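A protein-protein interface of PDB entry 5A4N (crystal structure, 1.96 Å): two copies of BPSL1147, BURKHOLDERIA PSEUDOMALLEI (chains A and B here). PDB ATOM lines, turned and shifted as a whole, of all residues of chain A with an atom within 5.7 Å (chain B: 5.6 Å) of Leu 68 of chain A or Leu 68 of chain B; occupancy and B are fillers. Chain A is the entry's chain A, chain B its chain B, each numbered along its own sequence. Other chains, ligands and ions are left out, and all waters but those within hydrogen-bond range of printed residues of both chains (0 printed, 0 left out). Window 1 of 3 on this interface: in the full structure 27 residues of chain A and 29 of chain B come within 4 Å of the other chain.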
ATOM      1  N   ILE A  23      32.389 -22.720  32.237  1.00  0.00           N
ATOM      2  CA  ILE A  23      31.599 -23.926  32.407  1.00  0.00           C
ATOM      3  C   ILE A  23      32.566 -25.062  32.550  1.00  0.00           C
ATOM      4  O   ILE A  23      33.360 -25.315  31.647  1.00  0.00           O
ATOM      5  CB  ILE A  23      30.682 -24.172  31.203  1.00  0.00           C
ATOM      6  CG1 ILE A  23      29.743 -22.988  31.068  1.00  0.00           C
ATOM      7  CG2 ILE A  23      29.899 -25.473  31.400  1.00  0.00           C
ATOM      8  CD1 ILE A  23      29.031 -22.917  29.793  1.00  0.00           C
ATOM      9  N   VAL A  34      28.040 -29.975  36.785  1.00  0.00           N
ATOM     10  CA  VAL A  34      28.388 -28.927  35.840  1.00  0.00           C
ATOM     11  C   VAL A  34      28.424 -27.568  36.561  1.00  0.00           C
ATOM     12  O   VAL A  34      27.438 -27.108  37.064  1.00  0.00           O
ATOM     13  CB  VAL A  34      27.387 -28.940  34.688  1.00  0.00           C
ATOM     14  CG1 VAL A  34      27.711 -27.822  33.721  1.00  0.00           C
ATOM     15  CG2 VAL A  34      27.477 -30.301  33.976  1.00  0.00           C
ATOM     16  N   VAL A  36      28.935 -23.643  36.570  1.00  0.00           N
ATOM     17  CA  VAL A  36      28.865 -22.487  35.706  1.00  0.00           C
ATOM     18  C   VAL A  36      29.225 -21.267  36.561  1.00  0.00           C
ATOM     19  O   VAL A  36      28.523 -20.959  37.486  1.00  0.00           O
ATOM     20  CB  VAL A  36      27.454 -22.334  35.163  1.00  0.00           C
ATOM     21  CG1 VAL A  36      27.418 -21.186  34.185  1.00  0.00           C
ATOM     22  CG2 VAL A  36      27.013 -23.641  34.508  1.00  0.00           C
ATOM     23  N   ILE A  56      25.217 -27.560  38.803  1.00  0.00           N
ATOM     24  CA  ILE A  56      24.073 -28.229  38.187  1.00  0.00           C
ATOM     25  C   ILE A  56      24.349 -29.723  38.155  1.00  0.00           C
ATOM     26  O   ILE A  56      25.285 -30.181  37.505  1.00  0.00           O
ATOM     27  CB  ILE A  56      23.818 -27.701  36.759  1.00  0.00           C
ATOM     28  CG1 ILE A  56      23.770 -26.173  36.768  1.00  0.00           C
ATOM     29  CG2 ILE A  56      22.531 -28.293  36.236  1.00  0.00           C
ATOM     30  CD1 ILE A  56      23.810 -25.531  35.408  1.00  0.00           C
ATOM     31  N   LEU A  61      20.375 -30.758  33.953  1.00  0.00           N
ATOM     32  CA  LEU A  61      21.022 -30.023  32.892  1.00  0.00           C
ATOM     33  C   LEU A  61      20.114 -29.857  31.687  1.00  0.00           C
ATOM     34  O   LEU A  61      19.989 -28.750  31.166  1.00  0.00           O
ATOM     35  CB  LEU A  61      22.311 -30.743  32.557  1.00  0.00           C
ATOM     36  CG  LEU A  61      23.386 -30.091  31.750  1.00  0.00           C
ATOM     37  CD1 LEU A  61      23.900 -28.811  32.351  1.00  0.00           C
ATOM     38  CD2 LEU A  61      24.502 -31.134  31.653  1.00  0.00           C
ATOM     39  N   GLN A  63      16.808 -29.604  31.615  1.00  0.00           N
ATOM     40  CA  GLN A  63      15.827 -28.576  31.953  1.00  0.00           C
ATOM     41  C   GLN A  63      16.422 -27.181  31.981  1.00  0.00           C
ATOM     42  O   GLN A  63      15.772 -26.228  31.581  1.00  0.00           O
ATOM     43  CB  GLN A  63      15.192 -28.876  33.289  1.00  0.00           C
ATOM     44  CG  GLN A  63      14.260 -30.065  33.247  1.00  0.00           C
ATOM     45  CD  GLN A  63      13.791 -30.411  34.660  1.00  0.00           C
ATOM     46  OE1 GLN A  63      14.321 -31.311  35.303  1.00  0.00           O
ATOM     47  NE2 GLN A  63      12.878 -29.612  35.170  1.00  0.00           N
ATOM     48  N   VAL A  64      17.658 -27.059  32.444  1.00  0.00           N
ATOM     49  CA  VAL A  64      18.312 -25.761  32.482  1.00  0.00           C
ATOM     50  C   VAL A  64      18.528 -25.254  31.051  1.00  0.00           C
ATOM     51  O   VAL A  64      18.235 -24.114  30.747  1.00  0.00           O
ATOM     52  CB  VAL A  64      19.620 -25.775  33.262  1.00  0.00           C
ATOM     53  CG1 VAL A  64      20.401 -24.501  33.041  1.00  0.00           C
ATOM     54  CG2 VAL A  64      19.355 -25.952  34.730  1.00  0.00           C
ATOM     55  N   ILE A  65      18.969 -26.128  30.165  1.00  0.00           N
ATOM     56  CA  ILE A  65      19.180 -25.743  28.743  1.00  0.00           C
ATOM     57  C   ILE A  65      17.845 -25.333  28.096  1.00  0.00           C
ATOM     58  O   ILE A  65      17.780 -24.341  27.387  1.00  0.00           O
ATOM     59  CB  ILE A  65      19.856 -26.880  27.978  1.00  0.00           C
ATOM     60  CG1 ILE A  65      21.287 -27.106  28.493  1.00  0.00           C
ATOM     61  CG2 ILE A  65      19.869 -26.598  26.490  1.00  0.00           C
ATOM     62  CD1 ILE A  65      21.876 -28.448  28.066  1.00  0.00           C
ATOM     63  N   GLN A  66      16.773 -26.069  28.348  1.00  0.00           N
ATOM     64  CA  GLN A  66      15.446 -25.724  27.756  1.00  0.00           C
ATOM     65  C   GLN A  66      14.990 -24.360  28.254  1.00  0.00           C
ATOM     66  O   GLN A  66      14.378 -23.592  27.522  1.00  0.00           O
ATOM     67  CB  GLN A  66      14.406 -26.759  28.151  1.00  0.00           C
ATOM     68  CG  GLN A  66      14.504 -28.039  27.340  1.00  0.00           C
ATOM     69  CD  GLN A  66      14.388 -27.762  25.836  1.00  0.00           C
ATOM     70  OE1 GLN A  66      13.379 -27.221  25.355  1.00  0.00           O
ATOM     71  NE2 GLN A  66      15.450 -28.093  25.089  1.00  0.00           N
ATOM     72  N   GLY A  67      15.280 -24.080  29.524  1.00  0.00           N
ATOM     73  CA  GLY A  67      15.017 -22.752  30.107  1.00  0.00           C
ATOM     74  C   GLY A  67      15.756 -21.640  29.407  1.00  0.00           C
ATOM     75  O   GLY A  67      15.161 -20.637  29.064  1.00  0.00           O
ATOM     76  N   LEU A  68      17.042 -21.836  29.155  1.00  0.00           N
ATOM     77  CA  LEU A  68      17.813 -20.866  28.388  1.00  0.00           C
ATOM     78  C   LEU A  68      17.357 -20.707  26.955  1.00  0.00           C
ATOM     79  O   LEU A  68      17.421 -19.593  26.400  1.00  0.00           O
ATOM     80  CB  LEU A  68      19.302 -21.222  28.401  1.00  0.00           C
ATOM     81  CG  LEU A  68      19.881 -21.177  29.807  1.00  0.00           C
ATOM     82  CD1 LEU A  68      21.296 -21.742  29.812  1.00  0.00           C
ATOM     83  CD2 LEU A  68      19.911 -19.774  30.335  1.00  0.00           C
ATOM     84  N   LEU A  69      16.855 -21.782  26.353  1.00  0.00           N
ATOM     85  CA  LEU A  69      16.343 -21.661  25.003  1.00  0.00           C
ATOM     86  C   LEU A  69      15.066 -20.828  25.049  1.00  0.00           C
ATOM     87  O   LEU A  69      14.876 -19.911  24.244  1.00  0.00           O
ATOM     88  CB  LEU A  69      16.081 -23.029  24.385  1.00  0.00           C
ATOM     89  CG  LEU A  69      17.355 -23.752  23.996  1.00  0.00           C
ATOM     90  CD1 LEU A  69      17.023 -25.196  23.666  1.00  0.00           C
ATOM     91  CD2 LEU A  69      18.012 -23.066  22.803  1.00  0.00           C
ATOM     92  N   LEU A  70      14.231 -21.102  26.026  1.00  0.00           N
ATOM     93  CA  LEU A  70      12.983 -20.346  26.170  1.00  0.00           C
ATOM     94  C   LEU A  70      13.318 -18.880  26.339  1.00  0.00           C
ATOM     95  O   LEU A  70      12.648 -18.022  25.805  1.00  0.00           O
ATOM     96  CB  LEU A  70      12.212 -20.890  27.357  1.00  0.00           C
ATOM     97  CG  LEU A  70      10.737 -20.641  27.452  1.00  0.00           C
ATOM     98  CD1 LEU A  70      10.063 -21.057  26.160  1.00  0.00           C
ATOM     99  CD2 LEU A  70      10.179 -21.395  28.668  1.00  0.00           C
ATOM    100  N   ALA A  71      14.402 -18.603  27.057  1.00  0.00           N
ATOM    101  CA  ALA A  71      14.804 -17.249  27.361  1.00  0.00           C
ATOM    102  C   ALA A  71      15.448 -16.578  26.179  1.00  0.00           C
ATOM    103  O   ALA A  71      15.664 -15.367  26.238  1.00  0.00           O
ATOM    104  CB  ALA A  71      15.767 -17.224  28.558  1.00  0.00           C
ATOM    105  N   SER A  72      15.793 -17.339  25.122  1.00  0.00           N
ATOM    106  CA  SER A  72      16.416 -16.747  23.928  1.00  0.00           C
ATOM    107  C   SER A  72      15.420 -15.884  23.147  1.00  0.00           C
ATOM    108  O   SER A  72      14.224 -16.192  23.120  1.00  0.00           O
ATOM    109  CB  SER A  72      16.992 -17.815  22.980  1.00  0.00           C
ATOM    110  OG  SER A  72      17.996 -18.606  23.629  1.00  0.00           O
ATOM    111  N   ILE B  23      15.713 -19.334  35.796  1.00  0.00           N
ATOM    112  CA  ILE B  23      16.182 -18.595  34.626  1.00  0.00           C
ATOM    113  C   ILE B  23      15.230 -17.411  34.465  1.00  0.00           C
ATOM    114  O   ILE B  23      14.010 -17.597  34.420  1.00  0.00           O
ATOM    115  CB  ILE B  23      16.180 -19.467  33.375  1.00  0.00           C
ATOM    116  CG1 ILE B  23      17.204 -20.612  33.499  1.00  0.00           C
ATOM    117  CG2 ILE B  23      16.498 -18.652  32.131  1.00  0.00           C
ATOM    118  CD1 ILE B  23      16.584 -21.940  33.857  1.00  0.00           C
ATOM    119  N   VAL B  34      20.130 -12.190  30.614  1.00  0.00           N
ATOM    120  CA  VAL B  34      19.561 -13.464  31.016  1.00  0.00           C
ATOM    121  C   VAL B  34      20.302 -13.875  32.284  1.00  0.00           C
ATOM    122  O   VAL B  34      21.510 -13.861  32.311  1.00  0.00           O
ATOM    123  CB  VAL B  34      19.702 -14.541  29.964  1.00  0.00           C
ATOM    124  CG1 VAL B  34      19.051 -15.841  30.411  1.00  0.00           C
ATOM    125  CG2 VAL B  34      19.010 -14.099  28.714  1.00  0.00           C
ATOM    126  N   VAL B  36      20.788 -16.710  35.455  1.00  0.00           N
ATOM    127  CA  VAL B  36      20.562 -18.074  35.905  1.00  0.00           C
ATOM    128  C   VAL B  36      21.073 -18.148  37.337  1.00  0.00           C
ATOM    129  O   VAL B  36      22.236 -17.903  37.548  1.00  0.00           O
ATOM    130  CB  VAL B  36      21.339 -19.098  35.048  1.00  0.00           C
ATOM    131  CG1 VAL B  36      20.979 -20.516  35.444  1.00  0.00           C
ATOM    132  CG2 VAL B  36      21.017 -18.890  33.612  1.00  0.00           C
ATOM    133  N   ILE B  56      24.150 -12.912  31.871  1.00  0.00           N
ATOM    134  CA  ILE B  56      24.648 -13.218  30.540  1.00  0.00           C
ATOM    135  C   ILE B  56      23.997 -12.169  29.647  1.00  0.00           C
ATOM    136  O   ILE B  56      22.787 -12.155  29.558  1.00  0.00           O
ATOM    137  CB  ILE B  56      24.117 -14.619  30.087  1.00  0.00           C
ATOM    138  CG1 ILE B  56      24.476 -15.713  31.080  1.00  0.00           C
ATOM    139  CG2 ILE B  56      24.636 -15.013  28.759  1.00  0.00           C
ATOM    140  CD1 ILE B  56      23.704 -17.052  30.995  1.00  0.00           C
ATOM    141  N   LEU B  61      24.557 -15.796  25.047  1.00  0.00           N
ATOM    142  CA  LEU B  61      23.699 -16.889  25.436  1.00  0.00           C
ATOM    143  C   LEU B  61      23.971 -18.134  24.581  1.00  0.00           C
ATOM    144  O   LEU B  61      24.074 -19.230  25.116  1.00  0.00           O
ATOM    145  CB  LEU B  61      22.257 -16.436  25.372  1.00  0.00           C
ATOM    146  CG  LEU B  61      21.147 -17.338  25.831  1.00  0.00           C
ATOM    147  CD1 LEU B  61      21.400 -17.725  27.265  1.00  0.00           C
ATOM    148  CD2 LEU B  61      19.800 -16.651  25.673  1.00  0.00           C
ATOM    149  N   GLN B  63      26.733 -19.218  23.347  1.00  0.00           N
ATOM    150  CA  GLN B  63      27.947 -19.905  23.816  1.00  0.00           C
ATOM    151  C   GLN B  63      27.733 -20.602  25.144  1.00  0.00           C
ATOM    152  O   GLN B  63      28.337 -21.637  25.399  1.00  0.00           O
ATOM    153  CB  GLN B  63      29.082 -18.935  23.993  1.00  0.00           C
ATOM    154  CG  GLN B  63      29.718 -18.495  22.719  1.00  0.00           C
ATOM    155  CD  GLN B  63      30.769 -17.450  22.995  1.00  0.00           C
ATOM    156  OE1 GLN B  63      31.860 -17.750  23.498  1.00  0.00           O
ATOM    157  NE2 GLN B  63      30.427 -16.213  22.711  1.00  0.00           N
ATOM    158  N   VAL B  64      26.903 -20.025  26.015  1.00  0.00           N
ATOM    159  CA  VAL B  64      26.567 -20.691  27.280  1.00  0.00           C
ATOM    160  C   VAL B  64      25.764 -21.971  27.043  1.00  0.00           C
ATOM    161  O   VAL B  64      26.141 -23.030  27.570  1.00  0.00           O
ATOM    162  CB  VAL B  64      25.842 -19.778  28.251  1.00  0.00           C
ATOM    163  CG1 VAL B  64      25.315 -20.565  29.473  1.00  0.00           C
ATOM    164  CG2 VAL B  64      26.747 -18.611  28.629  1.00  0.00           C
ATOM    165  N   ILE B  65      24.741 -21.894  26.190  1.00  0.00           N
ATOM    166  CA  ILE B  65      23.986 -23.084  25.752  1.00  0.00           C
ATOM    167  C   ILE B  65      24.902 -24.158  25.158  1.00  0.00           C
ATOM    168  O   ILE B  65      24.821 -25.323  25.548  1.00  0.00           O
ATOM    169  CB  ILE B  65      22.858 -22.710  24.782  1.00  0.00           C
ATOM    170  CG1 ILE B  65      21.809 -21.931  25.585  1.00  0.00           C
ATOM    171  CG2 ILE B  65      22.169 -23.911  24.191  1.00  0.00           C
ATOM    172  CD1 ILE B  65      20.770 -21.273  24.771  1.00  0.00           C
ATOM    173  N   GLN B  66      25.826 -23.768  24.292  1.00  0.00           N
ATOM    174  CA  GLN B  66      26.731 -24.728  23.680  1.00  0.00           C
ATOM    175  C   GLN B  66      27.629 -25.420  24.738  1.00  0.00           C
ATOM    176  O   GLN B  66      27.807 -26.629  24.716  1.00  0.00           O
ATOM    177  CB  GLN B  66      27.585 -24.033  22.659  1.00  0.00           C
ATOM    178  CG  GLN B  66      28.502 -24.987  21.886  1.00  0.00           C
ATOM    179  CD  GLN B  66      29.607 -24.282  21.148  1.00  0.00           C
ATOM    180  OE1 GLN B  66      30.118 -23.266  21.584  1.00  0.00           O
ATOM    181  NE2 GLN B  66      30.005 -24.836  20.054  1.00  0.00           N
ATOM    182  N   GLY B  67      28.142 -24.646  25.675  1.00  0.00           N
ATOM    183  CA  GLY B  67      28.951 -25.158  26.775  1.00  0.00           C
ATOM    184  C   GLY B  67      28.208 -26.165  27.601  1.00  0.00           C
ATOM    185  O   GLY B  67      28.745 -27.225  27.950  1.00  0.00           O
ATOM    186  N   LEU B  68      26.971 -25.855  27.915  1.00  0.00           N
ATOM    187  CA  LEU B  68      26.167 -26.747  28.719  1.00  0.00           C
ATOM    188  C   LEU B  68      25.883 -28.048  27.976  1.00  0.00           C
ATOM    189  O   LEU B  68      25.907 -29.120  28.576  1.00  0.00           O
ATOM    190  CB  LEU B  68      24.875 -26.065  29.171  1.00  0.00           C
ATOM    191  CG  LEU B  68      25.056 -24.965  30.223  1.00  0.00           C
ATOM    192  CD1 LEU B  68      23.738 -24.285  30.460  1.00  0.00           C
ATOM    193  CD2 LEU B  68      25.672 -25.440  31.563  1.00  0.00           C
ATOM    194  N   LEU B  69      25.623 -27.956  26.673  1.00  0.00           N
ATOM    195  CA  LEU B  69      25.409 -29.141  25.866  1.00  0.00           C
ATOM    196  C   LEU B  69      26.658 -30.005  25.803  1.00  0.00           C
ATOM    197  O   LEU B  69      26.601 -31.210  25.905  1.00  0.00           O
ATOM    198  CB  LEU B  69      24.975 -28.705  24.467  1.00  0.00           C
ATOM    199  CG  LEU B  69      23.555 -28.255  24.396  1.00  0.00           C
ATOM    200  CD1 LEU B  69      23.315 -27.411  23.157  1.00  0.00           C
ATOM    201  CD2 LEU B  69      22.649 -29.485  24.401  1.00  0.00           C
ATOM    202  N   LEU B  70      27.803 -29.367  25.642  1.00  0.00           N
ATOM    203  CA  LEU B  70      29.040 -30.072  25.621  1.00  0.00           C
ATOM    204  C   LEU B  70      29.296 -30.710  26.966  1.00  0.00           C
ATOM    205  O   LEU B  70      29.879 -31.769  27.010  1.00  0.00           O
ATOM    206  CB  LEU B  70      30.184 -29.121  25.265  1.00  0.00           C
ATOM    207  CG  LEU B  70      30.196 -28.671  23.783  1.00  0.00           C
ATOM    208  CD1 LEU B  70      31.201 -27.536  23.622  1.00  0.00           C
ATOM    209  CD2 LEU B  70      30.515 -29.812  22.815  1.00  0.00           C
ATOM    210  N   ALA B  71      28.869 -30.061  28.046  1.00  0.00           N
ATOM    211  CA  ALA B  71      29.057 -30.602  29.370  1.00  0.00           C
ATOM    212  C   ALA B  71      28.211 -31.835  29.667  1.00  0.00           C
ATOM    213  O   ALA B  71      28.470 -32.504  30.653  1.00  0.00           O
ATOM    214  CB  ALA B  71      28.805 -29.521  30.410  1.00  0.00           C
ATOM    215  N   SER B  72      27.191 -32.107  28.852  1.00  0.00           N
ATOM    216  CA  SER B  72      26.347 -33.301  28.984  1.00  0.00           C
ATOM    217  C   SER B  72      27.105 -34.559  28.632  1.00  0.00           C
ATOM    218  O   SER B  72      26.811 -35.635  29.134  1.00  0.00           O
ATOM    219  CB  SER B  72      25.131 -33.205  28.032  1.00  0.00           C
ATOM    220  OG  SER B  72      24.382 -32.024  28.316  1.00  0.00           O
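Val 36 of chain A touches Leu 68 of chain B, and with the chains exchanged Leu 68 of chain A touches Val 36 of chain B.
Ile 65 of chain A touches Leu 69 of chain B, and with the chains exchanged Leu 69 of chain A touches Ile 65 of chain B.
Leu 68 of chain A touches its own counterpart, Leu 68 of chain B.
Ala 71 of chain A touches Ile 23 of chain B, but with the chains exchanged Ile 23 of chain A does not touch Ala 71 of chain B (4.3 Å).
15 positions are printed for both chains.
Of the 17 pairs that touch across the chains among the printed residues, 13 have their exchanged pair printed and touching as well.
Hydrophobic or aromatic side chains of chain A that line the printed part of chain B: Ile 23, Val 34, Val 36, Leu 61, Ile 65, Leu 68, Leu 69 and Ala 71.
Printed residues of chain B that touch a printed residue of chain A: Ile 23, Val 36, Leu 61, Val 64, Ile 65, Gly 67, Leu 68, Leu 69, Ala 71 and Ser 72.
Hydrophobic or aromatic side chains of chain B within 4 Å of the printed part of chain A: Ile 23, Val 36, Leu 61, Ile 65, Leu 68, Leu 69 and Ala 71.
Along chain B the printed residues that touch a printed residue of chain A span positions 23 to 72.
The backbone carbonyl oxygen of Leu 69 of chain A sits close to the side-chain hydroxyl of Ser 72 of chain A, 3.4 Å away.
O of Leu 68 of chain B is in hydrogen-bond range of OG of Ser 72 of chain B.
The backbone carbonyl oxygen of Leu 68 of chain A lies within hydrogen-bond range of the side-chain hydroxyl of Ser 72 of chain A, 3.0 Å away.
The backbone carbonyl oxygen (O) of Ile 56 of chain A sits at hydrogen-bond distance from the backbone NH (N) of Val 34 of chain A (2.9 Å).
The backbone carbonyl oxygen (O) of Leu 69 of chain B lies close to the side-chain hydroxyl (OG) of Ser 72 of chain B (3.4 Å).
Printed residues of chain B within 4 Å of Val 34 of chain A: Leu 68 and Ala 71.
Of the printed residues of chain B, Leu 68 of chain A touches Val 36, Leu 61, Ile 65 and Leu 68.
Of the printed residues of chain B, Leu 69 of chain A touches Ile 65.
Of the printed residues of chain A, Ile 23 of chain B touches Gly 67 and Ala 71.
Gln 63 of chain B touches none of the printed residues of chain A.
Of the printed residues of chain A, Ala 71 of chain B touches Val 34 (3.9 Å).
The nearest printed residue of chain B that does not touch Leu 68 of chain A is Ile 23 of chain B (4.02 Å).
The nearest residue of chain A that does not touch Leu 68 of chain B is Ile 23 of chain A (4.05 Å).
The nearest printed residue of chain A that does not touch Leu 69 of chain B is Leu 61 of chain A (5.9 Å).
Among the printed residues, pairs that only touch across the chains: Ile 23 of chain A with Val 64 of chain B, Ile 23 of chain A with Gly 67 of chain B, Val 34 of chain A with Leu 68 of chain B, Val 34 of chain A with Ala 71 of chain B, Val 36 of chain A with Leu 68 of chain B, Leu 61 of chain A with Leu 68 of chain B, Leu 61 of chain A with Ser 72 of chain B, Ile 65 of chain A with Leu 68 of chain B, Ile 65 of chain A with Leu 69 of chain B, Gly 67 of chain A with Ile 23 of chain B, Leu 68 of chain A with Val 36 of chain B, Leu 68 of chain A with Leu 61 of chain B, Leu 68 of chain A with Ile 65 of chain B, Leu 68 of chain A with Leu 68 of chain B, Leu 69 of chain A with Ile 65 of chain B, Ala 71 of chain A with Ile 23 of chain B and Ser 72 of chain A with Leu 61 of chain B.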
